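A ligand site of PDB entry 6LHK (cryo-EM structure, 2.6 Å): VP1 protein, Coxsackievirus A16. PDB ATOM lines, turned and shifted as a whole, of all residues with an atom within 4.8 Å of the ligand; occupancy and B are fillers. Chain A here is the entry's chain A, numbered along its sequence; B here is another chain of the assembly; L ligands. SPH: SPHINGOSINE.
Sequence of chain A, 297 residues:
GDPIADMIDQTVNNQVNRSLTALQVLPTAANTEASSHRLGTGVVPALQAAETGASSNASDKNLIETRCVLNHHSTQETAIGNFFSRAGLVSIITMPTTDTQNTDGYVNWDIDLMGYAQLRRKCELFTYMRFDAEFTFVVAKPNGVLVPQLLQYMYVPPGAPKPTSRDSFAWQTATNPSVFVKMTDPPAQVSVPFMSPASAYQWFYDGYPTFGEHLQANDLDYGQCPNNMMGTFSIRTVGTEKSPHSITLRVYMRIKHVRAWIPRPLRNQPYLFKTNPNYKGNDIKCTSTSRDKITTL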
ATOM      1  N   ILE A 111      31.512   0.729  -8.955  1.00  0.00           N
ATOM      2  CA  ILE A 111      30.579   1.794  -9.297  1.00  0.00           C
ATOM      3  C   ILE A 111      30.374   2.746  -8.133  1.00  0.00           C
ATOM      4  O   ILE A 111      29.714   2.411  -7.143  1.00  0.00           O
ATOM      5  CB  ILE A 111      29.227   1.224  -9.762  1.00  0.00           C
ATOM      6  CG1 ILE A 111      29.418   0.251 -10.924  1.00  0.00           C
ATOM      7  CG2 ILE A 111      28.289   2.347 -10.179  1.00  0.00           C
ATOM      8  CD1 ILE A 111      28.168  -0.492 -11.300  1.00  0.00           C
ATOM      9  N   ASP A 112      30.945   3.940  -8.245  1.00  0.00           N
ATOM     10  CA  ASP A 112      30.716   5.025  -7.291  1.00  0.00           C
ATOM     11  C   ASP A 112      30.665   6.315  -8.097  1.00  0.00           C
ATOM     12  O   ASP A 112      31.679   6.747  -8.646  1.00  0.00           O
ATOM     13  CB  ASP A 112      31.808   5.078  -6.230  1.00  0.00           C
ATOM     14  CG  ASP A 112      31.527   6.102  -5.151  1.00  0.00           C
ATOM     15  OD1 ASP A 112      30.464   5.992  -4.496  1.00  0.00           O
ATOM     16  OD2 ASP A 112      32.350   7.005  -4.949  1.00  0.00           O
ATOM     17  N   LEU A 113      29.497   6.944  -8.146  1.00  0.00           N
ATOM     18  CA  LEU A 113      29.251   8.067  -9.036  1.00  0.00           C
ATOM     19  C   LEU A 113      29.432   9.420  -8.353  1.00  0.00           C
ATOM     20  O   LEU A 113      28.879  10.427  -8.810  1.00  0.00           O
ATOM     21  CB  LEU A 113      27.844   7.954  -9.640  1.00  0.00           C
ATOM     22  CG  LEU A 113      27.496   6.583 -10.204  1.00  0.00           C
ATOM     23  CD1 LEU A 113      26.055   6.556 -10.651  1.00  0.00           C
ATOM     24  CD2 LEU A 113      28.417   6.213 -11.346  1.00  0.00           C
ATOM     25  N   MET A 114      30.189   9.460  -7.262  1.00  0.00           N
ATOM     26  CA  MET A 114      30.400  10.683  -6.498  1.00  0.00           C
ATOM     27  C   MET A 114      31.809  11.216  -6.664  1.00  0.00           C
ATOM     28  O   MET A 114      32.381  11.790  -5.734  1.00  0.00           O
ATOM     29  CB  MET A 114      30.083  10.450  -5.017  1.00  0.00           C
ATOM     30  CG  MET A 114      28.642  10.066  -4.731  1.00  0.00           C
ATOM     31  SD  MET A 114      27.466  11.428  -4.861  1.00  0.00           S
ATOM     32  CE  MET A 114      26.617  11.032  -6.382  1.00  0.00           C
ATOM     33  N   PHE A 131      15.166   7.192  -8.859  1.00  0.00           N
ATOM     34  CA  PHE A 131      15.129   7.509 -10.278  1.00  0.00           C
ATOM     35  C   PHE A 131      15.560   6.306 -11.114  1.00  0.00           C
ATOM     36  O   PHE A 131      16.188   5.364 -10.616  1.00  0.00           O
ATOM     37  CB  PHE A 131      16.002   8.717 -10.612  1.00  0.00           C
ATOM     38  CG  PHE A 131      17.424   8.627 -10.096  1.00  0.00           C
ATOM     39  CD1 PHE A 131      18.418   8.025 -10.859  1.00  0.00           C
ATOM     40  CD2 PHE A 131      17.772   9.177  -8.875  1.00  0.00           C
ATOM     41  CE1 PHE A 131      19.714   7.954 -10.400  1.00  0.00           C
ATOM     42  CE2 PHE A 131      19.067   9.106  -8.417  1.00  0.00           C
ATOM     43  CZ  PHE A 131      20.038   8.495  -9.180  1.00  0.00           C
ATOM     44  N   PHE A 135      22.679   5.623 -19.249  1.00  0.00           N
ATOM     45  CA  PHE A 135      24.135   5.709 -19.278  1.00  0.00           C
ATOM     46  C   PHE A 135      24.627   5.742 -20.717  1.00  0.00           C
ATOM     47  O   PHE A 135      24.169   4.964 -21.545  1.00  0.00           O
ATOM     48  CB  PHE A 135      24.760   4.529 -18.525  1.00  0.00           C
ATOM     49  CG  PHE A 135      24.734   4.690 -17.037  1.00  0.00           C
ATOM     50  CD1 PHE A 135      23.662   4.240 -16.295  1.00  0.00           C
ATOM     51  CD2 PHE A 135      25.787   5.288 -16.378  1.00  0.00           C
ATOM     52  CE1 PHE A 135      23.637   4.382 -14.931  1.00  0.00           C
ATOM     53  CE2 PHE A 135      25.771   5.440 -15.008  1.00  0.00           C
ATOM     54  CZ  PHE A 135      24.685   4.983 -14.285  1.00  0.00           C
ATOM     55  N   PHE A 137      28.231   5.865 -23.137  1.00  0.00           N
ATOM     56  CA  PHE A 137      29.633   5.460 -23.080  1.00  0.00           C
ATOM     57  C   PHE A 137      30.374   6.055 -24.275  1.00  0.00           C
ATOM     58  O   PHE A 137      30.268   5.549 -25.390  1.00  0.00           O
ATOM     59  CB  PHE A 137      29.755   3.936 -23.060  1.00  0.00           C
ATOM     60  CG  PHE A 137      28.965   3.292 -21.959  1.00  0.00           C
ATOM     61  CD1 PHE A 137      29.482   3.188 -20.683  1.00  0.00           C
ATOM     62  CD2 PHE A 137      27.694   2.797 -22.202  1.00  0.00           C
ATOM     63  CE1 PHE A 137      28.763   2.601 -19.677  1.00  0.00           C
ATOM     64  CE2 PHE A 137      26.962   2.220 -21.190  1.00  0.00           C
ATOM     65  CZ  PHE A 137      27.496   2.117 -19.928  1.00  0.00           C
ATOM     66  N   TYR A 153      31.572  -4.188 -22.648  1.00  0.00           N
ATOM     67  CA  TYR A 153      31.233  -3.660 -21.330  1.00  0.00           C
ATOM     68  C   TYR A 153      30.307  -4.660 -20.658  1.00  0.00           C
ATOM     69  O   TYR A 153      29.330  -5.095 -21.266  1.00  0.00           O
ATOM     70  CB  TYR A 153      30.551  -2.297 -21.406  1.00  0.00           C
ATOM     71  CG  TYR A 153      31.129  -1.288 -22.374  1.00  0.00           C
ATOM     72  CD1 TYR A 153      32.507  -1.119 -22.509  1.00  0.00           C
ATOM     73  CD2 TYR A 153      30.299  -0.476 -23.123  1.00  0.00           C
ATOM     74  CE1 TYR A 153      33.023  -0.189 -23.381  1.00  0.00           C
ATOM     75  CE2 TYR A 153      30.801   0.454 -23.990  1.00  0.00           C
ATOM     76  CZ  TYR A 153      32.166   0.603 -24.122  1.00  0.00           C
ATOM     77  OH  TYR A 153      32.678   1.532 -24.984  1.00  0.00           O
ATOM     78  N   TYR A 155      28.165  -5.480 -16.904  1.00  0.00           N
ATOM     79  CA  TYR A 155      27.743  -5.082 -15.571  1.00  0.00           C
ATOM     80  C   TYR A 155      27.777  -6.294 -14.644  1.00  0.00           C
ATOM     81  O   TYR A 155      27.132  -7.315 -14.917  1.00  0.00           O
ATOM     82  CB  TYR A 155      26.333  -4.489 -15.603  1.00  0.00           C
ATOM     83  CG  TYR A 155      25.733  -4.262 -14.224  1.00  0.00           C
ATOM     84  CD1 TYR A 155      26.417  -3.533 -13.272  1.00  0.00           C
ATOM     85  CD2 TYR A 155      24.486  -4.775 -13.903  1.00  0.00           C
ATOM     86  CE1 TYR A 155      25.884  -3.325 -12.018  1.00  0.00           C
ATOM     87  CE2 TYR A 155      23.944  -4.567 -12.653  1.00  0.00           C
ATOM     88  CZ  TYR A 155      24.646  -3.836 -11.715  1.00  0.00           C
ATOM     89  OH  TYR A 155      24.109  -3.627 -10.474  1.00  0.00           O
ATOM     90  N   PRO A 177      24.271  -8.756 -17.887  1.00  0.00           N
ATOM     91  CA  PRO A 177      24.028  -7.915 -19.067  1.00  0.00           C
ATOM     92  C   PRO A 177      25.329  -7.341 -19.612  1.00  0.00           C
ATOM     93  O   PRO A 177      26.158  -6.825 -18.866  1.00  0.00           O
ATOM     94  CB  PRO A 177      23.093  -6.818 -18.543  1.00  0.00           C
ATOM     95  CG  PRO A 177      23.328  -6.782 -17.088  1.00  0.00           C
ATOM     96  CD  PRO A 177      23.702  -8.163 -16.660  1.00  0.00           C
ATOM     97  N   VAL A 179      27.334  -5.415 -23.231  1.00  0.00           N
ATOM     98  CA  VAL A 179      27.249  -4.662 -24.478  1.00  0.00           C
ATOM     99  C   VAL A 179      28.538  -4.866 -25.265  1.00  0.00           C
ATOM    100  O   VAL A 179      29.632  -4.638 -24.731  1.00  0.00           O
ATOM    101  CB  VAL A 179      27.009  -3.161 -24.245  1.00  0.00           C
ATOM    102  CG1 VAL A 179      26.787  -2.447 -25.560  1.00  0.00           C
ATOM    103  CG2 VAL A 179      25.827  -2.932 -23.327  1.00  0.00           C
ATOM    104  N   VAL A 190      22.231   2.744 -22.744  1.00  0.00           N
ATOM    105  CA  VAL A 190      21.393   1.745 -22.097  1.00  0.00           C
ATOM    106  C   VAL A 190      20.522   2.436 -21.059  1.00  0.00           C
ATOM    107  O   VAL A 190      20.834   3.513 -20.560  1.00  0.00           O
ATOM    108  CB  VAL A 190      22.209   0.610 -21.439  1.00  0.00           C
ATOM    109  CG1 VAL A 190      22.789  -0.314 -22.480  1.00  0.00           C
ATOM    110  CG2 VAL A 190      23.286   1.185 -20.549  1.00  0.00           C
ATOM    111  N   VAL A 192      18.823   1.953 -17.277  1.00  0.00           N
ATOM    112  CA  VAL A 192      19.085   1.265 -16.019  1.00  0.00           C
ATOM    113  C   VAL A 192      17.938   1.590 -15.066  1.00  0.00           C
ATOM    114  O   VAL A 192      17.607   2.758 -14.905  1.00  0.00           O
ATOM    115  CB  VAL A 192      20.432   1.669 -15.406  1.00  0.00           C
ATOM    116  CG1 VAL A 192      20.635   1.051 -14.035  1.00  0.00           C
ATOM    117  CG2 VAL A 192      21.568   1.261 -16.327  1.00  0.00           C
ATOM    118  N   MET A 195      17.405   0.157  -8.683  1.00  0.00           N
ATOM    119  CA  MET A 195      17.800  -1.158  -8.217  1.00  0.00           C
ATOM    120  C   MET A 195      18.359  -1.137  -6.799  1.00  0.00           C
ATOM    121  O   MET A 195      19.282  -1.898  -6.478  1.00  0.00           O
ATOM    122  CB  MET A 195      18.805  -1.800  -9.177  1.00  0.00           C
ATOM    123  CG  MET A 195      19.983  -0.930  -9.532  1.00  0.00           C
ATOM    124  SD  MET A 195      21.122  -1.828 -10.585  1.00  0.00           S
ATOM    125  CE  MET A 195      20.118  -2.076 -12.032  1.00  0.00           C
ATOM    126  N   TYR A 201      17.628   5.942  -3.070  1.00  0.00           N
ATOM    127  CA  TYR A 201      19.041   6.139  -2.799  1.00  0.00           C
ATOM    128  C   TYR A 201      19.213   7.279  -1.795  1.00  0.00           C
ATOM    129  O   TYR A 201      18.518   8.301  -1.874  1.00  0.00           O
ATOM    130  CB  TYR A 201      19.819   6.479  -4.065  1.00  0.00           C
ATOM    131  CG  TYR A 201      19.706   5.492  -5.194  1.00  0.00           C
ATOM    132  CD1 TYR A 201      20.136   4.178  -5.044  1.00  0.00           C
ATOM    133  CD2 TYR A 201      19.201   5.882  -6.427  1.00  0.00           C
ATOM    134  CE1 TYR A 201      20.041   3.280  -6.078  1.00  0.00           C
ATOM    135  CE2 TYR A 201      19.097   4.986  -7.465  1.00  0.00           C
ATOM    136  CZ  TYR A 201      19.519   3.690  -7.295  1.00  0.00           C
ATOM    137  OH  TYR A 201      19.424   2.793  -8.329  1.00  0.00           O
ATOM    138  N   GLN A 202      20.135   7.108  -0.856  1.00  0.00           N
ATOM    139  CA  GLN A 202      20.459   8.182   0.069  1.00  0.00           C
ATOM    140  C   GLN A 202      21.927   8.563  -0.106  1.00  0.00           C
ATOM    141  O   GLN A 202      22.807   7.702  -0.069  1.00  0.00           O
ATOM    142  CB  GLN A 202      20.187   7.799   1.525  1.00  0.00           C
ATOM    143  CG  GLN A 202      20.519   6.385   1.897  1.00  0.00           C
ATOM    144  CD  GLN A 202      20.054   6.052   3.300  1.00  0.00           C
ATOM    145  OE1 GLN A 202      20.072   6.907   4.184  1.00  0.00           O
ATOM    146  NE2 GLN A 202      19.637   4.806   3.502  1.00  0.00           N
ATOM    147  N   TRP A 203      22.170   9.855  -0.307  1.00  0.00           N
ATOM    148  CA  TRP A 203      23.531  10.351  -0.400  1.00  0.00           C
ATOM    149  C   TRP A 203      24.166  10.578   0.961  1.00  0.00           C
ATOM    150  O   TRP A 203      25.377  10.810   1.030  1.00  0.00           O
ATOM    151  CB  TRP A 203      23.569  11.639  -1.208  1.00  0.00           C
ATOM    152  CG  TRP A 203      22.555  11.687  -2.301  1.00  0.00           C
ATOM    153  CD1 TRP A 203      21.471  12.486  -2.362  1.00  0.00           C
ATOM    154  CD2 TRP A 203      22.520  10.873  -3.477  1.00  0.00           C
ATOM    155  NE1 TRP A 203      20.757  12.240  -3.506  1.00  0.00           N
ATOM    156  CE2 TRP A 203      21.385  11.249  -4.209  1.00  0.00           C
ATOM    157  CE3 TRP A 203      23.346   9.858  -3.989  1.00  0.00           C
ATOM    158  CZ2 TRP A 203      21.051  10.658  -5.417  1.00  0.00           C
ATOM    159  CZ3 TRP A 203      23.007   9.276  -5.187  1.00  0.00           C
ATOM    160  CH2 TRP A 203      21.873   9.679  -5.894  1.00  0.00           C
ATOM    161  N   ASN A 228      23.369   1.563  -1.542  1.00  0.00           N
ATOM    162  CA  ASN A 228      23.810   2.314  -2.709  1.00  0.00           C
ATOM    163  C   ASN A 228      24.904   1.611  -3.489  1.00  0.00           C
ATOM    164  O   ASN A 228      25.218   2.048  -4.599  1.00  0.00           O
ATOM    165  CB  ASN A 228      24.306   3.707  -2.295  1.00  0.00           C
ATOM    166  CG  ASN A 228      23.286   4.477  -1.497  1.00  0.00           C
ATOM    167  OD1 ASN A 228      23.552   4.899  -0.381  1.00  0.00           O
ATOM    168  ND2 ASN A 228      22.111   4.667  -2.076  1.00  0.00           N
ATOM    169  N   MET A 230      26.281  -0.809  -5.941  1.00  0.00           N
ATOM    170  CA  MET A 230      25.608  -1.440  -7.068  1.00  0.00           C
ATOM    171  C   MET A 230      26.462  -2.441  -7.832  1.00  0.00           C
ATOM    172  O   MET A 230      25.956  -3.088  -8.749  1.00  0.00           O
ATOM    173  CB  MET A 230      25.082  -0.373  -8.028  1.00  0.00           C
ATOM    174  CG  MET A 230      23.874   0.359  -7.499  1.00  0.00           C
ATOM    175  SD  MET A 230      22.585  -0.813  -7.024  1.00  0.00           S
ATOM    176  CE  MET A 230      21.942  -0.030  -5.559  1.00  0.00           C
ATOM    177  N   PHE A 233      31.643  -2.444 -12.770  1.00  0.00           N
ATOM    178  CA  PHE A 233      31.539  -2.254 -14.209  1.00  0.00           C
ATOM    179  C   PHE A 233      32.872  -2.667 -14.839  1.00  0.00           C
ATOM    180  O   PHE A 233      33.920  -2.105 -14.508  1.00  0.00           O
ATOM    181  CB  PHE A 233      31.197  -0.805 -14.528  1.00  0.00           C
ATOM    182  CG  PHE A 233      31.109  -0.513 -15.984  1.00  0.00           C
ATOM    183  CD1 PHE A 233      30.065  -1.011 -16.741  1.00  0.00           C
ATOM    184  CD2 PHE A 233      32.072   0.269 -16.603  1.00  0.00           C
ATOM    185  CE1 PHE A 233      29.988  -0.741 -18.083  1.00  0.00           C
ATOM    186  CE2 PHE A 233      31.995   0.539 -17.945  1.00  0.00           C
ATOM    187  CZ  PHE A 233      30.956   0.039 -18.689  1.00  0.00           C
ATOM    188  N   ILE B  24      18.370  -2.916 -19.790  1.00  0.00           N
ATOM    189  CA  ILE B  24      19.341  -3.974 -19.529  1.00  0.00           C
ATOM    190  C   ILE B  24      18.770  -5.180 -18.797  1.00  0.00           C
ATOM    191  O   ILE B  24      19.379  -6.257 -18.852  1.00  0.00           O
ATOM    192  CB  ILE B  24      20.554  -3.423 -18.743  1.00  0.00           C
ATOM    193  CG1 ILE B  24      20.114  -2.781 -17.429  1.00  0.00           C
ATOM    194  CG2 ILE B  24      21.327  -2.444 -19.567  1.00  0.00           C
ATOM    195  CD1 ILE B  24      21.201  -2.694 -16.401  1.00  0.00           C
HETATM  196  C1  SPH L   1      27.235   6.198  -3.810  1.00  0.00           C
HETATM  197  O1  SPH L   1      27.022   7.178  -2.814  1.00  0.00           O
HETATM  198  C2  SPH L   1      25.981   6.046  -4.657  1.00  0.00           C
HETATM  199  N2  SPH L   1      24.970   6.933  -4.121  1.00  0.00           N
HETATM  200  C3  SPH L   1      26.274   6.389  -6.118  1.00  0.00           C
HETATM  201  O3  SPH L   1      27.570   5.913  -6.416  1.00  0.00           O
HETATM  202  C4  SPH L   1      25.289   5.768  -7.069  1.00  0.00           C
HETATM  203  C5  SPH L   1      24.067   5.072  -6.641  1.00  0.00           C
HETATM  204  C6  SPH L   1      23.273   4.259  -7.631  1.00  0.00           C
HETATM  205  C7  SPH L   1      23.074   5.002  -8.943  1.00  0.00           C
HETATM  206  C8  SPH L   1      22.587   4.071 -10.043  1.00  0.00           C
HETATM  207  C9  SPH L   1      23.543   2.900 -10.242  1.00  0.00           C
HETATM  208  C10 SPH L   1      23.471   2.300 -11.637  1.00  0.00           C
HETATM  209  C11 SPH L   1      24.587   1.287 -11.847  1.00  0.00           C
HETATM  210  C12 SPH L   1      24.295   0.348 -13.011  1.00  0.00           C
HETATM  211  C13 SPH L   1      24.977   0.813 -14.290  1.00  0.00           C
HETATM  212  C14 SPH L   1      25.349  -0.373 -15.186  1.00  0.00           C
HETATM  213  C15 SPH L   1      25.636   0.088 -16.617  1.00  0.00           C
HETATM  214  C16 SPH L   1      26.290  -1.012 -17.439  1.00  0.00           C
HETATM  215  C17 SPH L   1      25.312  -1.639 -18.432  1.00  0.00           C
HETATM  216  C18 SPH L   1      26.032  -2.562 -19.418  1.00  0.00           C
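An oxygen (O3) of the ligand is in hydrogen-bond range of the backbone NH (N) of Leu 113, 2.8 Å away. The side-chain carboxylate of Asp 112 lies close to an oxygen (O3) of the ligand.
Merely in contact with the ligand: Met 114 (3.8 Å), Phe 135 (3.9 Å), Tyr 155 (3.8 Å), Val 179 (3.9 Å), Val 192 (3.9 Å), Tyr 201 (3.7 Å), Trp 203 (3.2 Å), Asn 228 (3.7 Å), Met 230 (3.8 Å) and Phe 233 (3.8 Å). 12 residues have an atom within 4 Å of the ligand: Asp 112, Leu 113, Met 114, Phe 135, Tyr 155, Val 179, Val 192, Tyr 201, Trp 203, Asn 228, Met 230 and Phe 233. The nearest printed residue that does not touch the ligand is Ile 111 (4.04 Å).
The backbone NH (N) of Met 195 sits at hydrogen-bond distance from the side-chain hydroxyl (OH) of Tyr 201 (3.3 Å). OD1 of Asn 228 lies close to O of Gln 202, 2.9 Å away. O of Met 230 lies within hydrogen-bond range of OH of Tyr 155. N of Tyr 155 lies within hydrogen-bond range of O of Pro 177, at 3.1 Å. The side-chain sulfur (SD) of Met 195 lies within hydrogen-bond range of the side-chain hydroxyl (OH) of Tyr 155. O of Val 190 is in hydrogen-bond range of N of Phe 135 (3.1 Å). The backbone NH (N) of Val 179 is in hydrogen-bond range of the backbone carbonyl oxygen (O) of Tyr 153, 2.8 Å away.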
